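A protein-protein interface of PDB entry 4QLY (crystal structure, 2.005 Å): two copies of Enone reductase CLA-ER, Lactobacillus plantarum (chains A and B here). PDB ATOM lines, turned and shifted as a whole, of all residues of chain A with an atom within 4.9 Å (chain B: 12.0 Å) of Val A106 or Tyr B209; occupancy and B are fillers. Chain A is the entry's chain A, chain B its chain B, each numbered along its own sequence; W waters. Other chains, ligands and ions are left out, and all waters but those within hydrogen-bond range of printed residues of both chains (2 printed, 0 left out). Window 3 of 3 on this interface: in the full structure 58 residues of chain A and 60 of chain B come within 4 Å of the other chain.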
ATOM      1  N   LEU A  55       6.233  11.790 -27.760  1.00  0.00           N
ATOM      2  CA  LEU A  55       6.141  11.431 -26.353  1.00  0.00           C
ATOM      3  C   LEU A  55       4.846  10.717 -25.981  1.00  0.00           C
ATOM      4  O   LEU A  55       4.769  10.111 -24.910  1.00  0.00           O
ATOM      5  CB  LEU A  55       6.304  12.670 -25.484  1.00  0.00           C
ATOM      6  CG  LEU A  55       7.642  13.394 -25.599  1.00  0.00           C
ATOM      7  CD1 LEU A  55       7.648  14.517 -24.582  1.00  0.00           C
ATOM      8  CD2 LEU A  55       8.821  12.444 -25.383  1.00  0.00           C
ATOM      9  N   GLN A  56       3.835  10.791 -26.848  1.00  0.00           N
ATOM     10  CA  GLN A  56       2.614  10.002 -26.668  1.00  0.00           C
ATOM     11  C   GLN A  56       2.049  10.145 -25.258  1.00  0.00           C
ATOM     12  O   GLN A  56       1.702   9.150 -24.615  1.00  0.00           O
ATOM     13  CB  GLN A  56       2.889   8.527 -26.963  1.00  0.00           C
ATOM     14  CG  GLN A  56       3.486   8.278 -28.356  1.00  0.00           C
ATOM     15  CD  GLN A  56       4.190   6.931 -28.438  1.00  0.00           C
ATOM     16  OE1 GLN A  56       3.553   5.881 -28.314  1.00  0.00           O
ATOM     17  NE2 GLN A  56       5.517   6.959 -28.631  1.00  0.00           N
ATOM     18  N   SER A  99       5.774  12.420 -19.089  1.00  0.00           N
ATOM     19  CA  SER A  99       5.980  11.500 -20.213  1.00  0.00           C
ATOM     20  C   SER A  99       7.385  11.586 -20.789  1.00  0.00           C
ATOM     21  O   SER A  99       7.837  10.667 -21.455  1.00  0.00           O
ATOM     22  CB  SER A  99       4.975  11.767 -21.337  1.00  0.00           C
ATOM     23  OG  SER A  99       5.234  13.012 -21.957  1.00  0.00           O
ATOM     24  N   VAL A 102       9.379   9.007 -18.983  1.00  0.00           N
ATOM     25  CA  VAL A 102       9.053   7.679 -19.494  1.00  0.00           C
ATOM     26  C   VAL A 102       9.864   7.419 -20.758  1.00  0.00           C
ATOM     27  O   VAL A 102      10.481   6.365 -20.926  1.00  0.00           O
ATOM     28  CB  VAL A 102       7.550   7.532 -19.808  1.00  0.00           C
ATOM     29  CG1 VAL A 102       7.255   6.136 -20.366  1.00  0.00           C
ATOM     30  CG2 VAL A 102       6.722   7.810 -18.558  1.00  0.00           C
ATOM     31  N   TYR A 103       9.862   8.406 -21.644  1.00  0.00           N
ATOM     32  CA  TYR A 103      10.594   8.318 -22.903  1.00  0.00           C
ATOM     33  C   TYR A 103      12.075   8.107 -22.633  1.00  0.00           C
ATOM     34  O   TYR A 103      12.701   7.211 -23.208  1.00  0.00           O
ATOM     35  CB  TYR A 103      10.366   9.585 -23.734  1.00  0.00           C
ATOM     36  CG  TYR A 103      10.501   9.377 -25.225  1.00  0.00           C
ATOM     37  CD1 TYR A 103       9.779   8.386 -25.877  1.00  0.00           C
ATOM     38  CD2 TYR A 103      11.346  10.179 -25.982  1.00  0.00           C
ATOM     39  CE1 TYR A 103       9.900   8.195 -27.241  1.00  0.00           C
ATOM     40  CE2 TYR A 103      11.472  10.002 -27.354  1.00  0.00           C
ATOM     41  CZ  TYR A 103      10.751   9.010 -27.974  1.00  0.00           C
ATOM     42  OH  TYR A 103      10.879   8.832 -29.329  1.00  0.00           O
ATOM     43  N   ARG A 104      12.619   8.924 -21.735  1.00  0.00           N
ATOM     44  CA  ARG A 104      14.019   8.803 -21.329  1.00  0.00           C
ATOM     45  C   ARG A 104      14.355   7.408 -20.792  1.00  0.00           C
ATOM     46  O   ARG A 104      15.366   6.811 -21.180  1.00  0.00           O
ATOM     47  CB  ARG A 104      14.361   9.843 -20.267  1.00  0.00           C
ATOM     48  CG  ARG A 104      15.786   9.678 -19.712  1.00  0.00           C
ATOM     49  CD  ARG A 104      15.896  10.191 -18.282  1.00  0.00           C
ATOM     50  NE  ARG A 104      14.995   9.465 -17.389  1.00  0.00           N
ATOM     51  CZ  ARG A 104      14.745   9.823 -16.135  1.00  0.00           C
ATOM     52  NH1 ARG A 104      15.332  10.900 -15.626  1.00  0.00           N
ATOM     53  NH2 ARG A 104      13.913   9.105 -15.393  1.00  0.00           N
ATOM     54  N   ASP A 105      13.502   6.899 -19.905  1.00  0.00           N
ATOM     55  CA  ASP A 105      13.727   5.599 -19.271  1.00  0.00           C
ATOM     56  C   ASP A 105      13.843   4.494 -20.303  1.00  0.00           C
ATOM     57  O   ASP A 105      14.663   3.591 -20.156  1.00  0.00           O
ATOM     58  CB  ASP A 105      12.609   5.266 -18.283  1.00  0.00           C
ATOM     59  CG  ASP A 105      12.619   6.172 -17.067  1.00  0.00           C
ATOM     60  OD1 ASP A 105      13.591   6.950 -16.913  1.00  0.00           O
ATOM     61  OD2 ASP A 105      11.657   6.102 -16.267  1.00  0.00           O
ATOM     62  N   VAL A 106      13.027   4.573 -21.348  1.00  0.00           N
ATOM     63  CA  VAL A 106      13.094   3.608 -22.437  1.00  0.00           C
ATOM     64  C   VAL A 106      14.498   3.540 -23.035  1.00  0.00           C
ATOM     65  O   VAL A 106      15.086   2.453 -23.139  1.00  0.00           O
ATOM     66  CB  VAL A 106      12.095   3.948 -23.547  1.00  0.00           C
ATOM     67  CG1 VAL A 106      12.374   3.106 -24.798  1.00  0.00           C
ATOM     68  CG2 VAL A 106      10.683   3.735 -23.054  1.00  0.00           C
ATOM     69  N   TRP A 107      15.040   4.704 -23.393  1.00  0.00           N
ATOM     70  CA  TRP A 107      16.339   4.771 -24.049  1.00  0.00           C
ATOM     71  C   TRP A 107      17.462   4.383 -23.090  1.00  0.00           C
ATOM     72  O   TRP A 107      18.402   3.699 -23.492  1.00  0.00           O
ATOM     73  CB  TRP A 107      16.583   6.176 -24.634  1.00  0.00           C
ATOM     74  CG  TRP A 107      15.468   6.626 -25.539  1.00  0.00           C
ATOM     75  CD1 TRP A 107      14.658   7.720 -25.372  1.00  0.00           C
ATOM     76  CD2 TRP A 107      15.016   5.976 -26.733  1.00  0.00           C
ATOM     77  NE1 TRP A 107      13.741   7.795 -26.396  1.00  0.00           N
ATOM     78  CE2 TRP A 107      13.934   6.733 -27.240  1.00  0.00           C
ATOM     79  CE3 TRP A 107      15.415   4.826 -27.422  1.00  0.00           C
ATOM     80  CZ2 TRP A 107      13.260   6.379 -28.404  1.00  0.00           C
ATOM     81  CZ3 TRP A 107      14.739   4.477 -28.577  1.00  0.00           C
ATOM     82  CH2 TRP A 107      13.676   5.253 -29.058  1.00  0.00           C
ATOM     83  N   ASN A 108      17.360   4.826 -21.835  1.00  0.00           N
ATOM     84  CA  ASN A 108      18.345   4.475 -20.814  1.00  0.00           C
ATOM     85  C   ASN A 108      18.511   2.963 -20.722  1.00  0.00           C
ATOM     86  O   ASN A 108      19.616   2.460 -20.552  1.00  0.00           O
ATOM     87  CB  ASN A 108      17.945   5.020 -19.435  1.00  0.00           C
ATOM     88  CG  ASN A 108      18.331   6.475 -19.230  1.00  0.00           C
ATOM     89  OD1 ASN A 108      18.997   7.088 -20.066  1.00  0.00           O
ATOM     90  ND2 ASN A 108      17.929   7.030 -18.087  1.00  0.00           N
ATOM     91  N   LYS A 109      17.396   2.247 -20.832  1.00  0.00           N
ATOM     92  CA  LYS A 109      17.404   0.796 -20.697  1.00  0.00           C
ATOM     93  C   LYS A 109      18.169   0.153 -21.839  1.00  0.00           C
ATOM     94  O   LYS A 109      18.937  -0.789 -21.629  1.00  0.00           O
ATOM     95  CB  LYS A 109      15.975   0.241 -20.645  1.00  0.00           C
ATOM     96  CG  LYS A 109      15.188   0.647 -19.411  1.00  0.00           C
ATOM     97  CD  LYS A 109      16.052   0.614 -18.159  1.00  0.00           C
ATOM     98  CE  LYS A 109      15.197   0.709 -16.891  1.00  0.00           C
ATOM     99  NZ  LYS A 109      14.145   1.762 -16.998  1.00  0.00           N
ATOM    100  N   VAL A 110      17.941   0.660 -23.048  1.00  0.00           N
ATOM    101  CA  VAL A 110      18.648   0.177 -24.230  1.00  0.00           C
ATOM    102  C   VAL A 110      20.152   0.338 -24.055  1.00  0.00           C
ATOM    103  O   VAL A 110      20.935  -0.556 -24.402  1.00  0.00           O
ATOM    104  CB  VAL A 110      18.206   0.925 -25.495  1.00  0.00           C
ATOM    105  CG1 VAL A 110      19.049   0.489 -26.696  1.00  0.00           C
ATOM    106  CG2 VAL A 110      16.731   0.690 -25.747  1.00  0.00           C
ATOM    107  N   ARG B  22      -0.718   7.485 -41.759  1.00  0.00           N
ATOM    108  CA  ARG B  22      -0.378   8.897 -41.653  1.00  0.00           C
ATOM    109  C   ARG B  22       0.986   9.035 -40.997  1.00  0.00           C
ATOM    110  O   ARG B  22       1.203   8.507 -39.911  1.00  0.00           O
ATOM    111  CB  ARG B  22      -1.423   9.667 -40.833  1.00  0.00           C
ATOM    112  CG  ARG B  22      -1.038  11.117 -40.560  1.00  0.00           C
ATOM    113  CD  ARG B  22      -1.480  11.602 -39.160  1.00  0.00           C
ATOM    114  NE  ARG B  22      -0.847  10.803 -38.109  1.00  0.00           N
ATOM    115  CZ  ARG B  22       0.418  10.929 -37.715  1.00  0.00           C
ATOM    116  NH1 ARG B  22       1.216  11.821 -38.283  1.00  0.00           N
ATOM    117  NH2 ARG B  22       0.903  10.139 -36.760  1.00  0.00           N
ATOM    118  N   HIS B 205      10.534   7.123 -39.886  1.00  0.00           N
ATOM    119  CA  HIS B 205       9.821   6.061 -39.204  1.00  0.00           C
ATOM    120  C   HIS B 205       9.722   6.368 -37.715  1.00  0.00           C
ATOM    121  O   HIS B 205      10.690   6.839 -37.108  1.00  0.00           O
ATOM    122  CB  HIS B 205      10.530   4.718 -39.419  1.00  0.00           C
ATOM    123  CG  HIS B 205      10.482   4.226 -40.835  1.00  0.00           C
ATOM    124  ND1 HIS B 205      10.544   5.072 -41.921  1.00  0.00           N
ATOM    125  CD2 HIS B 205      10.384   2.972 -41.337  1.00  0.00           C
ATOM    126  CE1 HIS B 205      10.477   4.359 -43.035  1.00  0.00           C
ATOM    127  NE2 HIS B 205      10.379   3.084 -42.707  1.00  0.00           N
ATOM    128  N   THR B 206       8.555   6.116 -37.128  1.00  0.00           N
ATOM    129  CA  THR B 206       8.417   6.194 -35.677  1.00  0.00           C
ATOM    130  C   THR B 206       7.717   4.950 -35.144  1.00  0.00           C
ATOM    131  O   THR B 206       7.046   4.232 -35.886  1.00  0.00           O
ATOM    132  CB  THR B 206       7.629   7.434 -35.235  1.00  0.00           C
ATOM    133  OG1 THR B 206       6.319   7.387 -35.803  1.00  0.00           O
ATOM    134  CG2 THR B 206       8.329   8.716 -35.695  1.00  0.00           C
ATOM    135  N   THR B 207       7.874   4.703 -33.851  1.00  0.00           N
ATOM    136  CA  THR B 207       7.155   3.619 -33.201  1.00  0.00           C
ATOM    137  C   THR B 207       6.168   4.197 -32.203  1.00  0.00           C
ATOM    138  O   THR B 207       6.217   5.388 -31.902  1.00  0.00           O
ATOM    139  CB  THR B 207       8.100   2.662 -32.456  1.00  0.00           C
ATOM    140  OG1 THR B 207       8.871   3.409 -31.508  1.00  0.00           O
ATOM    141  CG2 THR B 207       9.036   1.967 -33.418  1.00  0.00           C
ATOM    142  N   ARG B 208       5.292   3.344 -31.685  1.00  0.00           N
ATOM    143  CA  ARG B 208       4.434   3.691 -30.562  1.00  0.00           C
ATOM    144  C   ARG B 208       4.630   2.699 -29.437  1.00  0.00           C
ATOM    145  O   ARG B 208       4.986   1.545 -29.693  1.00  0.00           O
ATOM    146  CB  ARG B 208       2.962   3.690 -30.968  1.00  0.00           C
ATOM    147  CG  ARG B 208       2.592   4.714 -32.026  1.00  0.00           C
ATOM    148  CD  ARG B 208       2.715   6.134 -31.519  1.00  0.00           C
ATOM    149  NE  ARG B 208       2.250   7.097 -32.525  1.00  0.00           N
ATOM    150  CZ  ARG B 208       2.983   7.524 -33.557  1.00  0.00           C
ATOM    151  NH1 ARG B 208       4.232   7.088 -33.743  1.00  0.00           N
ATOM    152  NH2 ARG B 208       2.470   8.404 -34.403  1.00  0.00           N
ATOM    153  N   TYR B 209       4.398   3.139 -28.201  1.00  0.00           N
ATOM    154  CA  TYR B 209       4.303   2.206 -27.079  1.00  0.00           C
ATOM    155  C   TYR B 209       3.247   1.168 -27.369  1.00  0.00           C
ATOM    156  O   TYR B 209       2.288   1.408 -28.118  1.00  0.00           O
ATOM    157  CB  TYR B 209       3.939   2.911 -25.762  1.00  0.00           C
ATOM    158  CG  TYR B 209       4.974   3.887 -25.263  1.00  0.00           C
ATOM    159  CD1 TYR B 209       6.192   3.443 -24.773  1.00  0.00           C
ATOM    160  CD2 TYR B 209       4.732   5.256 -25.278  1.00  0.00           C
ATOM    161  CE1 TYR B 209       7.135   4.331 -24.306  1.00  0.00           C
ATOM    162  CE2 TYR B 209       5.673   6.154 -24.823  1.00  0.00           C
ATOM    163  CZ  TYR B 209       6.875   5.691 -24.342  1.00  0.00           C
ATOM    164  OH  TYR B 209       7.820   6.592 -23.880  1.00  0.00           O
ATOM    165  N   ASP B 210       3.440   0.005 -26.771  1.00  0.00           N
ATOM    166  CA  ASP B 210       2.358  -0.937 -26.554  1.00  0.00           C
ATOM    167  C   ASP B 210       1.298  -0.201 -25.735  1.00  0.00           C
ATOM    168  O   ASP B 210       1.559   0.189 -24.595  1.00  0.00           O
ATOM    169  CB  ASP B 210       2.891  -2.178 -25.822  1.00  0.00           C
ATOM    170  CG  ASP B 210       1.838  -3.253 -25.635  1.00  0.00           C
ATOM    171  OD1 ASP B 210       0.624  -2.932 -25.591  1.00  0.00           O
ATOM    172  OD2 ASP B 210       2.241  -4.431 -25.522  1.00  0.00           O
ATOM    173  N   ALA B 211       0.119   0.012 -26.311  1.00  0.00           N
ATOM    174  CA  ALA B 211      -0.889   0.861 -25.661  1.00  0.00           C
ATOM    175  C   ALA B 211      -1.352   0.304 -24.308  1.00  0.00           C
ATOM    176  O   ALA B 211      -1.916   1.034 -23.493  1.00  0.00           O
ATOM    177  CB  ALA B 211      -2.086   1.063 -26.583  1.00  0.00           C
ATOM    178  N   LYS B 212      -1.071  -0.973 -24.042  1.00  0.00           N
ATOM    179  CA  LYS B 212      -1.437  -1.549 -22.751  1.00  0.00           C
ATOM    180  C   LYS B 212      -0.626  -0.907 -21.620  1.00  0.00           C
ATOM    181  O   LYS B 212      -1.068  -0.883 -20.476  1.00  0.00           O
ATOM    182  CB  LYS B 212      -1.256  -3.069 -22.759  1.00  0.00           C
ATOM    183  CG  LYS B 212      -2.240  -3.814 -23.655  1.00  0.00           C
ATOM    184  CD  LYS B 212      -1.951  -5.328 -23.657  1.00  0.00           C
ATOM    185  CE  LYS B 212      -1.976  -5.908 -22.243  1.00  0.00           C
ATOM    186  NZ  LYS B 212      -3.346  -5.968 -21.624  1.00  0.00           N
ATOM    187  N   THR B 213       0.549  -0.365 -21.937  1.00  0.00           N
ATOM    188  CA  THR B 213       1.360   0.288 -20.906  1.00  0.00           C
ATOM    189  C   THR B 213       0.737   1.594 -20.462  1.00  0.00           C
ATOM    190  O   THR B 213       1.098   2.135 -19.409  1.00  0.00           O
ATOM    191  CB  THR B 213       2.802   0.608 -21.372  1.00  0.00           C
ATOM    192  OG1 THR B 213       2.770   1.488 -22.508  1.00  0.00           O
ATOM    193  CG2 THR B 213       3.548  -0.639 -21.730  1.00  0.00           C
ATOM    194  N   GLN B 214      -0.174   2.113 -21.278  1.00  0.00           N
ATOM    195  CA  GLN B 214      -0.781   3.418 -21.015  1.00  0.00           C
ATOM    196  C   GLN B 214      -2.244   3.323 -20.598  1.00  0.00           C
ATOM    197  O   GLN B 214      -2.928   4.347 -20.482  1.00  0.00           O
ATOM    198  CB  GLN B 214      -0.661   4.299 -22.261  1.00  0.00           C
ATOM    199  CG  GLN B 214       0.766   4.451 -22.761  1.00  0.00           C
ATOM    200  CD  GLN B 214       0.836   5.221 -24.063  1.00  0.00           C
ATOM    201  OE1 GLN B 214       0.510   4.698 -25.132  1.00  0.00           O
ATOM    202  NE2 GLN B 214       1.261   6.473 -23.978  1.00  0.00           N
ATOM    203  N   THR B 215      -2.725   2.102 -20.389  1.00  0.00           N
ATOM    204  CA  THR B 215      -4.155   1.858 -20.176  1.00  0.00           C
ATOM    205  C   THR B 215      -4.448   1.212 -18.822  1.00  0.00           C
ATOM    206  O   THR B 215      -3.807   0.213 -18.446  1.00  0.00           O
ATOM    207  CB  THR B 215      -4.731   0.939 -21.294  1.00  0.00           C
ATOM    208  OG1 THR B 215      -4.464   1.503 -22.589  1.00  0.00           O
ATOM    209  CG2 THR B 215      -6.230   0.736 -21.121  1.00  0.00           C
HETATM  210  O   HOH W   1       0.885   5.336 -27.576  1.00  0.00           O
HETATM  211  O   HOH W   2       6.821   9.074 -23.365  1.00  0.00           O
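O of Tyr A103 lies close to NE1 of Trp A107 (3.4 Å).
The side-chain hydroxyl (OG1) of Thr B206 is in hydrogen-bond range of the guanidinium group (NH1) of Arg B208 (2.9 Å).
No position is printed for both chains.
Of the 7 pairs that touch across the chains among the printed residues, none has its exchanged pair printed and touching as well.
N of Tyr B209 is in hydrogen-bond range of OE1 of Gln A56 (2.9 Å).
The backbone carbonyl oxygen (O) of Gln A56 sits at hydrogen-bond distance from the side-chain amide nitrogen (NE2) of Gln B214, 2.8 Å away.
Val A106 touches just one residue of chain B: Tyr B209 (3.8 Å).
Of chain A, only Gln A56 (2.9 Å), Val A102 (3.6 Å), Tyr A103 (3.3 Å) and Val A106 (3.8 Å) come within 4 Å of Tyr B209.
Of chain B, only Thr B207, Arg B208, Tyr B209 and Gln B214 come within 4 Å of Gln A56.
No residue of chain B comes within 4 Å of Ser A99.
No residue of chain B comes within 4 Å of Asp A105.
No residue of chain B comes within 4 Å of Trp A107.
No residue of chain B comes within 4 Å of Asn A108.
No residue of chain B comes within 4 Å of Lys A109.
No residue of chain B comes within 4 Å of Val A110.
Of the printed residues of chain A, Gln B214 touches Gln A56 (2.8 Å).
Of the printed residues of chain A, Arg B208 touches Gln A56.
Printed residues of chain A within 4 Å of Thr B207: Gln A56 (3.7 Å).
The nearest residue of chain B that does not touch Val A106 is Thr B207 (7.6 Å).
The nearest residue of chain A that does not touch Tyr B209 is Leu A55 (4.1 Å).
Water W1 bridges the side-chain amide oxygen (OE1) of Gln B214 (2.6 Å) and the side-chain amide oxygen (OE1) of Gln A56 (2.8 Å).
Water W2 lies within hydrogen-bond range of O of Ser A99 (2.7 Å), OH of Tyr B209 (2.7 Å) and O of Leu A55 (2.8 Å).
Of the 12 printed residues of chain A, 4 touch a printed residue of chain B.
Hydrophobic or aromatic side chains of chain B within 4 Å of the printed part of chain A: Tyr B209.
Among the printed residues, 7 pairs touch across the chains.
Among the printed residues, no Asp or Glu carboxylate lies within 4 Å of a Lys or Arg side-chain nitrogen of the other chain.
Among the printed residues, merely in contact across the chains: Gln A56 with Arg B208, Tyr A103 with Tyr B209, Val A102 with Tyr B209, Gln A56 with Thr B207 and Val A106 with Tyr B209.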
